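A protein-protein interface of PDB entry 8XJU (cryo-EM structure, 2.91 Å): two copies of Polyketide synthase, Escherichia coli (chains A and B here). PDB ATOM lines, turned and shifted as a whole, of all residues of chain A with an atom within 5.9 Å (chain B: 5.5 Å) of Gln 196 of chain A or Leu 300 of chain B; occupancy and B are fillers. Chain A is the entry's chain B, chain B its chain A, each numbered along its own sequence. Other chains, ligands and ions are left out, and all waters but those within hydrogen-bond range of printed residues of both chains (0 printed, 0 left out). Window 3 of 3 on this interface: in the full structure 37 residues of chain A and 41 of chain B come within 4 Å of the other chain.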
ATOM      1  N   ASP A 116      15.044  -4.282 -31.733  1.00  0.00           N
ATOM      2  CA  ASP A 116      13.692  -4.116 -32.228  1.00  0.00           C
ATOM      3  C   ASP A 116      13.316  -2.651 -32.003  1.00  0.00           C
ATOM      4  O   ASP A 116      13.584  -2.113 -30.929  1.00  0.00           O
ATOM      5  CB  ASP A 116      12.806  -5.104 -31.463  1.00  0.00           C
ATOM      6  CG  ASP A 116      11.438  -5.223 -32.026  1.00  0.00           C
ATOM      7  OD1 ASP A 116      11.156  -4.530 -32.999  1.00  0.00           O
ATOM      8  OD2 ASP A 116      10.644  -6.028 -31.503  1.00  0.00           O
ATOM      9  N   GLY A 169       9.115  -2.745 -34.605  1.00  0.00           N
ATOM     10  CA  GLY A 169       8.532  -2.808 -33.292  1.00  0.00           C
ATOM     11  C   GLY A 169       7.170  -2.180 -33.314  1.00  0.00           C
ATOM     12  O   GLY A 169       6.615  -1.928 -34.382  1.00  0.00           O
ATOM     13  N   PRO A 170       6.610  -1.910 -32.134  1.00  0.00           N
ATOM     14  CA  PRO A 170       5.230  -1.421 -32.035  1.00  0.00           C
ATOM     15  C   PRO A 170       5.075  -0.041 -32.648  1.00  0.00           C
ATOM     16  O   PRO A 170       5.706   0.914 -32.207  1.00  0.00           O
ATOM     17  CB  PRO A 170       4.977  -1.390 -30.527  1.00  0.00           C
ATOM     18  CG  PRO A 170       6.086  -2.103 -29.908  1.00  0.00           C
ATOM     19  CD  PRO A 170       7.231  -2.053 -30.814  1.00  0.00           C
ATOM     20  N   GLN A 190       7.683   2.901 -21.537  1.00  0.00           N
ATOM     21  CA  GLN A 190       7.103   1.653 -21.051  1.00  0.00           C
ATOM     22  C   GLN A 190       7.418   0.484 -21.972  1.00  0.00           C
ATOM     23  O   GLN A 190       7.740  -0.602 -21.490  1.00  0.00           O
ATOM     24  CB  GLN A 190       5.594   1.784 -20.879  1.00  0.00           C
ATOM     25  CG  GLN A 190       5.209   2.832 -19.882  1.00  0.00           C
ATOM     26  CD  GLN A 190       3.900   2.563 -19.220  1.00  0.00           C
ATOM     27  OE1 GLN A 190       3.825   1.788 -18.272  1.00  0.00           O
ATOM     28  NE2 GLN A 190       2.851   3.203 -19.711  1.00  0.00           N
ATOM     29  N   SER A 191       7.340   0.694 -23.290  1.00  0.00           N
ATOM     30  CA  SER A 191       7.700  -0.356 -24.241  1.00  0.00           C
ATOM     31  C   SER A 191       9.162  -0.751 -24.131  1.00  0.00           C
ATOM     32  O   SER A 191       9.501  -1.927 -24.263  1.00  0.00           O
ATOM     33  CB  SER A 191       7.412   0.086 -25.658  1.00  0.00           C
ATOM     34  OG  SER A 191       6.034   0.017 -25.943  1.00  0.00           O
ATOM     35  N   LEU A 192      10.043   0.216 -23.916  1.00  0.00           N
ATOM     36  CA  LEU A 192      11.446  -0.105 -23.703  1.00  0.00           C
ATOM     37  C   LEU A 192      11.673  -0.861 -22.402  1.00  0.00           C
ATOM     38  O   LEU A 192      12.484  -1.788 -22.368  1.00  0.00           O
ATOM     39  CB  LEU A 192      12.281   1.166 -23.723  1.00  0.00           C
ATOM     40  CG  LEU A 192      12.652   1.669 -25.104  1.00  0.00           C
ATOM     41  CD1 LEU A 192      12.761   3.147 -25.068  1.00  0.00           C
ATOM     42  CD2 LEU A 192      13.956   1.059 -25.485  1.00  0.00           C
ATOM     43  N   LEU A 193      10.975  -0.496 -21.329  1.00  0.00           N
ATOM     44  CA  LEU A 193      11.218  -1.123 -20.036  1.00  0.00           C
ATOM     45  C   LEU A 193      10.459  -2.432 -19.828  1.00  0.00           C
ATOM     46  O   LEU A 193      10.810  -3.192 -18.922  1.00  0.00           O
ATOM     47  CB  LEU A 193      10.877  -0.138 -18.916  1.00  0.00           C
ATOM     48  CG  LEU A 193      11.819   1.062 -18.816  1.00  0.00           C
ATOM     49  CD1 LEU A 193      11.160   2.184 -18.071  1.00  0.00           C
ATOM     50  CD2 LEU A 193      13.119   0.682 -18.139  1.00  0.00           C
ATOM     51  N   THR A 194       9.444  -2.720 -20.636  1.00  0.00           N
ATOM     52  CA  THR A 194       8.866  -4.052 -20.708  1.00  0.00           C
ATOM     53  C   THR A 194       9.519  -4.903 -21.785  1.00  0.00           C
ATOM     54  O   THR A 194       9.072  -6.034 -22.009  1.00  0.00           O
ATOM     55  CB  THR A 194       7.354  -3.995 -20.973  1.00  0.00           C
ATOM     56  OG1 THR A 194       7.095  -3.374 -22.233  1.00  0.00           O
ATOM     57  CG2 THR A 194       6.638  -3.245 -19.886  1.00  0.00           C
ATOM     58  N   TRP A 195      10.550  -4.364 -22.451  1.00  0.00           N
ATOM     59  CA  TRP A 195      11.289  -5.010 -23.540  1.00  0.00           C
ATOM     60  C   TRP A 195      10.373  -5.365 -24.709  1.00  0.00           C
ATOM     61  O   TRP A 195      10.489  -6.429 -25.309  1.00  0.00           O
ATOM     62  CB  TRP A 195      12.067  -6.238 -23.054  1.00  0.00           C
ATOM     63  CG  TRP A 195      13.122  -5.964 -22.018  1.00  0.00           C
ATOM     64  CD1 TRP A 195      12.943  -5.426 -20.780  1.00  0.00           C
ATOM     65  CD2 TRP A 195      14.515  -6.260 -22.121  1.00  0.00           C
ATOM     66  NE1 TRP A 195      14.138  -5.342 -20.117  1.00  0.00           N
ATOM     67  CE2 TRP A 195      15.121  -5.850 -20.919  1.00  0.00           C
ATOM     68  CE3 TRP A 195      15.314  -6.822 -23.121  1.00  0.00           C
ATOM     69  CZ2 TRP A 195      16.486  -5.983 -20.688  1.00  0.00           C
ATOM     70  CZ3 TRP A 195      16.675  -6.954 -22.889  1.00  0.00           C
ATOM     71  CH2 TRP A 195      17.244  -6.536 -21.683  1.00  0.00           C
ATOM     72  N   GLN A 196       9.449  -4.466 -25.036  1.00  0.00           N
ATOM     73  CA  GLN A 196       8.708  -4.590 -26.283  1.00  0.00           C
ATOM     74  C   GLN A 196       9.528  -4.151 -27.482  1.00  0.00           C
ATOM     75  O   GLN A 196       9.165  -4.468 -28.621  1.00  0.00           O
ATOM     76  CB  GLN A 196       7.427  -3.760 -26.237  1.00  0.00           C
ATOM     77  CG  GLN A 196       6.285  -4.422 -25.510  1.00  0.00           C
ATOM     78  CD  GLN A 196       5.519  -5.377 -26.385  1.00  0.00           C
ATOM     79  OE1 GLN A 196       4.782  -4.963 -27.269  1.00  0.00           O
ATOM     80  NE2 GLN A 196       5.689  -6.668 -26.142  1.00  0.00           N
ATOM     81  N   CYS A 197      10.605  -3.408 -27.248  1.00  0.00           N
ATOM     82  CA  CYS A 197      11.487  -2.931 -28.297  1.00  0.00           C
ATOM     83  C   CYS A 197      12.831  -2.665 -27.651  1.00  0.00           C
ATOM     84  O   CYS A 197      12.945  -2.592 -26.428  1.00  0.00           O
ATOM     85  CB  CYS A 197      10.927  -1.684 -28.989  1.00  0.00           C
ATOM     86  SG  CYS A 197      10.332  -0.389 -27.911  1.00  0.00           S
ATOM     87  N   ASP A 198      13.859  -2.545 -28.483  1.00  0.00           N
ATOM     88  CA  ASP A 198      15.195  -2.260 -27.981  1.00  0.00           C
ATOM     89  C   ASP A 198      15.597  -0.807 -28.163  1.00  0.00           C
ATOM     90  O   ASP A 198      16.493  -0.331 -27.461  1.00  0.00           O
ATOM     91  CB  ASP A 198      16.219  -3.177 -28.653  1.00  0.00           C
ATOM     92  CG  ASP A 198      16.282  -4.539 -27.997  1.00  0.00           C
ATOM     93  OD1 ASP A 198      15.260  -4.969 -27.428  1.00  0.00           O
ATOM     94  OD2 ASP A 198      17.351  -5.180 -28.034  1.00  0.00           O
ATOM     95  N   ARG A 252      17.314   2.242 -23.674  1.00  0.00           N
ATOM     96  CA  ARG A 252      17.650   2.010 -22.282  1.00  0.00           C
ATOM     97  C   ARG A 252      19.075   2.463 -22.012  1.00  0.00           C
ATOM     98  O   ARG A 252      19.919   2.475 -22.903  1.00  0.00           O
ATOM     99  CB  ARG A 252      17.482   0.540 -21.941  1.00  0.00           C
ATOM    100  CG  ARG A 252      16.139  -0.006 -22.322  1.00  0.00           C
ATOM    101  CD  ARG A 252      15.945  -1.408 -21.798  1.00  0.00           C
ATOM    102  NE  ARG A 252      16.370  -2.423 -22.752  1.00  0.00           N
ATOM    103  CZ  ARG A 252      15.610  -2.902 -23.725  1.00  0.00           C
ATOM    104  NH1 ARG A 252      14.374  -2.465 -23.894  1.00  0.00           N
ATOM    105  NH2 ARG A 252      16.091  -3.826 -24.534  1.00  0.00           N
ATOM    106  N   GLN B 190       0.907  -3.071 -20.251  1.00  0.00           N
ATOM    107  CA  GLN B 190       2.164  -2.372 -19.981  1.00  0.00           C
ATOM    108  C   GLN B 190       2.035  -1.464 -18.770  1.00  0.00           C
ATOM    109  O   GLN B 190       2.840  -1.542 -17.836  1.00  0.00           O
ATOM    110  CB  GLN B 190       2.583  -1.535 -21.189  1.00  0.00           C
ATOM    111  CG  GLN B 190       3.312  -2.235 -22.313  1.00  0.00           C
ATOM    112  CD  GLN B 190       3.190  -1.465 -23.621  1.00  0.00           C
ATOM    113  OE1 GLN B 190       3.233  -0.239 -23.639  1.00  0.00           O
ATOM    114  NE2 GLN B 190       3.017  -2.186 -24.720  1.00  0.00           N
ATOM    115  N   LYS B 268      -0.902 -13.719 -19.792  1.00  0.00           N
ATOM    116  CA  LYS B 268       0.471 -14.048 -19.420  1.00  0.00           C
ATOM    117  C   LYS B 268       1.499 -13.380 -20.311  1.00  0.00           C
ATOM    118  O   LYS B 268       2.599 -13.069 -19.846  1.00  0.00           O
ATOM    119  CB  LYS B 268       0.684 -15.546 -19.437  1.00  0.00           C
ATOM    120  CG  LYS B 268      -0.150 -16.276 -18.461  1.00  0.00           C
ATOM    121  CD  LYS B 268       0.291 -15.930 -17.072  1.00  0.00           C
ATOM    122  CE  LYS B 268      -0.475 -16.709 -16.041  1.00  0.00           C
ATOM    123  NZ  LYS B 268      -0.064 -16.330 -14.668  1.00  0.00           N
ATOM    124  N   GLY B 269       1.184 -13.158 -21.575  1.00  0.00           N
ATOM    125  CA  GLY B 269       2.157 -12.528 -22.438  1.00  0.00           C
ATOM    126  C   GLY B 269       1.485 -11.878 -23.612  1.00  0.00           C
ATOM    127  O   GLY B 269       0.402 -12.278 -24.032  1.00  0.00           O
ATOM    128  N   PHE B 270       2.156 -10.877 -24.152  1.00  0.00           N
ATOM    129  CA  PHE B 270       1.601 -10.082 -25.227  1.00  0.00           C
ATOM    130  C   PHE B 270       2.752  -9.543 -26.054  1.00  0.00           C
ATOM    131  O   PHE B 270       3.889  -9.489 -25.591  1.00  0.00           O
ATOM    132  CB  PHE B 270       0.699  -8.954 -24.697  1.00  0.00           C
ATOM    133  CG  PHE B 270       1.391  -7.982 -23.779  1.00  0.00           C
ATOM    134  CD1 PHE B 270       1.547  -8.262 -22.432  1.00  0.00           C
ATOM    135  CD2 PHE B 270       1.862  -6.775 -24.262  1.00  0.00           C
ATOM    136  CE1 PHE B 270       2.178  -7.385 -21.610  1.00  0.00           C
ATOM    137  CE2 PHE B 270       2.486  -5.894 -23.432  1.00  0.00           C
ATOM    138  CZ  PHE B 270       2.639  -6.198 -22.108  1.00  0.00           C
ATOM    139  N   ALA B 271       2.449  -9.145 -27.283  1.00  0.00           N
ATOM    140  CA  ALA B 271       3.488  -8.677 -28.185  1.00  0.00           C
ATOM    141  C   ALA B 271       2.865  -7.856 -29.286  1.00  0.00           C
ATOM    142  O   ALA B 271       1.952  -8.324 -29.952  1.00  0.00           O
ATOM    143  CB  ALA B 271       4.250  -9.834 -28.800  1.00  0.00           C
ATOM    144  N   VAL B 272       3.372  -6.648 -29.481  1.00  0.00           N
ATOM    145  CA  VAL B 272       3.017  -5.798 -30.608  1.00  0.00           C
ATOM    146  C   VAL B 272       4.283  -5.550 -31.409  1.00  0.00           C
ATOM    147  O   VAL B 272       5.352  -5.334 -30.831  1.00  0.00           O
ATOM    148  CB  VAL B 272       2.387  -4.463 -30.151  1.00  0.00           C
ATOM    149  CG1 VAL B 272       1.800  -3.706 -31.317  1.00  0.00           C
ATOM    150  CG2 VAL B 272       1.328  -4.705 -29.130  1.00  0.00           C
ATOM    151  N   ALA B 295       5.402 -15.649 -31.413  1.00  0.00           N
ATOM    152  CA  ALA B 295       6.454 -16.276 -30.623  1.00  0.00           C
ATOM    153  C   ALA B 295       6.955 -15.382 -29.499  1.00  0.00           C
ATOM    154  O   ALA B 295       7.328 -15.888 -28.437  1.00  0.00           O
ATOM    155  CB  ALA B 295       7.615 -16.677 -31.524  1.00  0.00           C
ATOM    156  N   GLN B 296       6.935 -14.060 -29.692  1.00  0.00           N
ATOM    157  CA  GLN B 296       7.309 -13.131 -28.633  1.00  0.00           C
ATOM    158  C   GLN B 296       6.279 -13.118 -27.515  1.00  0.00           C
ATOM    159  O   GLN B 296       6.646 -13.078 -26.338  1.00  0.00           O
ATOM    160  CB  GLN B 296       7.481 -11.738 -29.223  1.00  0.00           C
ATOM    161  CG  GLN B 296       7.815 -10.657 -28.232  1.00  0.00           C
ATOM    162  CD  GLN B 296       7.764  -9.291 -28.869  1.00  0.00           C
ATOM    163  OE1 GLN B 296       7.329  -9.145 -30.008  1.00  0.00           O
ATOM    164  NE2 GLN B 296       8.200  -8.280 -28.137  1.00  0.00           N
ATOM    165  N   ALA B 297       4.988 -13.145 -27.868  1.00  0.00           N
ATOM    166  CA  ALA B 297       3.934 -13.233 -26.865  1.00  0.00           C
ATOM    167  C   ALA B 297       4.011 -14.533 -26.085  1.00  0.00           C
ATOM    168  O   ALA B 297       3.877 -14.531 -24.859  1.00  0.00           O
ATOM    169  CB  ALA B 297       2.573 -13.095 -27.532  1.00  0.00           C
ATOM    170  N   GLN B 298       4.258 -15.654 -26.767  1.00  0.00           N
ATOM    171  CA  GLN B 298       4.402 -16.921 -26.059  1.00  0.00           C
ATOM    172  C   GLN B 298       5.714 -17.026 -25.297  1.00  0.00           C
ATOM    173  O   GLN B 298       5.827 -17.864 -24.403  1.00  0.00           O
ATOM    174  CB  GLN B 298       4.282 -18.088 -27.029  1.00  0.00           C
ATOM    175  CG  GLN B 298       2.962 -18.173 -27.720  1.00  0.00           C
ATOM    176  CD  GLN B 298       2.980 -19.121 -28.877  1.00  0.00           C
ATOM    177  OE1 GLN B 298       4.013 -19.695 -29.210  1.00  0.00           O
ATOM    178  NE2 GLN B 298       1.832 -19.296 -29.508  1.00  0.00           N
ATOM    179  N   ARG B 299       6.711 -16.211 -25.635  1.00  0.00           N
ATOM    180  CA  ARG B 299       7.963 -16.213 -24.890  1.00  0.00           C
ATOM    181  C   ARG B 299       7.876 -15.372 -23.627  1.00  0.00           C
ATOM    182  O   ARG B 299       8.338 -15.801 -22.564  1.00  0.00           O
ATOM    183  CB  ARG B 299       9.091 -15.703 -25.781  1.00  0.00           C
ATOM    184  CG  ARG B 299      10.447 -15.737 -25.138  1.00  0.00           C
ATOM    185  CD  ARG B 299      11.478 -15.144 -26.059  1.00  0.00           C
ATOM    186  NE  ARG B 299      11.050 -13.877 -26.637  1.00  0.00           N
ATOM    187  CZ  ARG B 299      11.183 -12.701 -26.034  1.00  0.00           C
ATOM    188  NH1 ARG B 299      10.771 -11.596 -26.637  1.00  0.00           N
ATOM    189  NH2 ARG B 299      11.722 -12.631 -24.829  1.00  0.00           N
ATOM    190  N   LEU B 300       7.301 -14.165 -23.726  1.00  0.00           N
ATOM    191  CA  LEU B 300       7.026 -13.364 -22.535  1.00  0.00           C
ATOM    192  C   LEU B 300       5.977 -14.016 -21.655  1.00  0.00           C
ATOM    193  O   LEU B 300       5.969 -13.805 -20.441  1.00  0.00           O
ATOM    194  CB  LEU B 300       6.581 -11.958 -22.916  1.00  0.00           C
ATOM    195  CG  LEU B 300       7.533 -11.180 -23.809  1.00  0.00           C
ATOM    196  CD1 LEU B 300       6.868  -9.937 -24.322  1.00  0.00           C
ATOM    197  CD2 LEU B 300       8.783 -10.830 -23.046  1.00  0.00           C
ATOM    198  N   ALA B 301       5.098 -14.822 -22.242  1.00  0.00           N
ATOM    199  CA  ALA B 301       4.130 -15.600 -21.493  1.00  0.00           C
ATOM    200  C   ALA B 301       4.750 -16.738 -20.704  1.00  0.00           C
ATOM    201  O   ALA B 301       4.061 -17.327 -19.869  1.00  0.00           O
ATOM    202  CB  ALA B 301       3.090 -16.159 -22.446  1.00  0.00           C
ATOM    203  N   GLY B 302       6.015 -17.062 -20.947  1.00  0.00           N
ATOM    204  CA  GLY B 302       6.656 -18.193 -20.305  1.00  0.00           C
ATOM    205  C   GLY B 302       6.095 -19.517 -20.755  1.00  0.00           C
ATOM    206  O   GLY B 302       5.964 -20.437 -19.944  1.00  0.00           O
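O of Gln 190 of chain B sits close to OE1 of Gln 190 of chain A, 3.5 Å away. The side-chain amide nitrogen (NE2) of Gln 196 of chain A sits at hydrogen-bond distance from the backbone carbonyl oxygen (O) of Phe 270 of chain B. The backbone NH (N) of Val 272 of chain B sits at hydrogen-bond distance from the side-chain amide oxygen (OE1) of Gln 196 of chain A (3.1 Å).
Of the 14 printed residues of chain B, 6 touch a printed residue of chain A. Printed residues of chain B that touch a printed residue of chain A: Gln 190, Phe 270, Ala 271, Val 272, Gln 296 and Leu 300. Hydrophobic or aromatic side chains of chain B within 4 Å of the printed part of chain A: Val 272 and Leu 300. Of the 13 printed residues of chain A, 5 touch a printed residue of chain B. Printed residues of chain A that touch a printed residue of chain B: Pro 170, Gln 190, Ser 191, Thr 194 and Gln 196.
Gln 190 of chain B touches its own counterpart, Gln 190 of chain A. 1 position is printed for both chains. Of the 9 pairs that touch across the chains among the printed residues, 1 has its exchanged pair printed and touching as well.
Of the printed residues of chain B, Pro 170 of chain A touches Val 272. Of the printed residues of chain B, Ser 191 of chain A touches Gln 190 (3.6 Å). Gln 196 of chain A touches just these residues of chain B: Phe 270, Ala 271, Val 272, Gln 296 and Leu 300. Of chain A, only Gln 196 comes within 4 Å of Leu 300 of chain B.
The backbone carbonyl oxygen of Ser 191 of chain A sits at hydrogen-bond distance from the side-chain hydroxyl of Thr 194 of chain A, 3.5 Å away. The backbone carbonyl oxygen of Ser 191 of chain A lies within hydrogen-bond range of the backbone NH of Gln 196 of chain A, at 2.7 Å. The backbone carbonyl oxygen (O) of Gln 190 of chain A lies within hydrogen-bond range of the side-chain hydroxyl (OG1) of Thr 194 of chain A (2.9 Å).
Among the printed residues, merely in contact across the chains: Pro 170 of chain A with Val 272 of chain B (3.4 Å), Gln 196 of chain A with Gln 296 of chain B (3.6 Å), Gln 196 of chain A with Ala 271 of chain B (3.6 Å), Ser 191 of chain A with Gln 190 of chain B (3.6 Å), Gln 196 of chain A with Leu 300 of chain B (3.9 Å) and Thr 194 of chain A with Gln 190 of chain B (3.95 Å).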
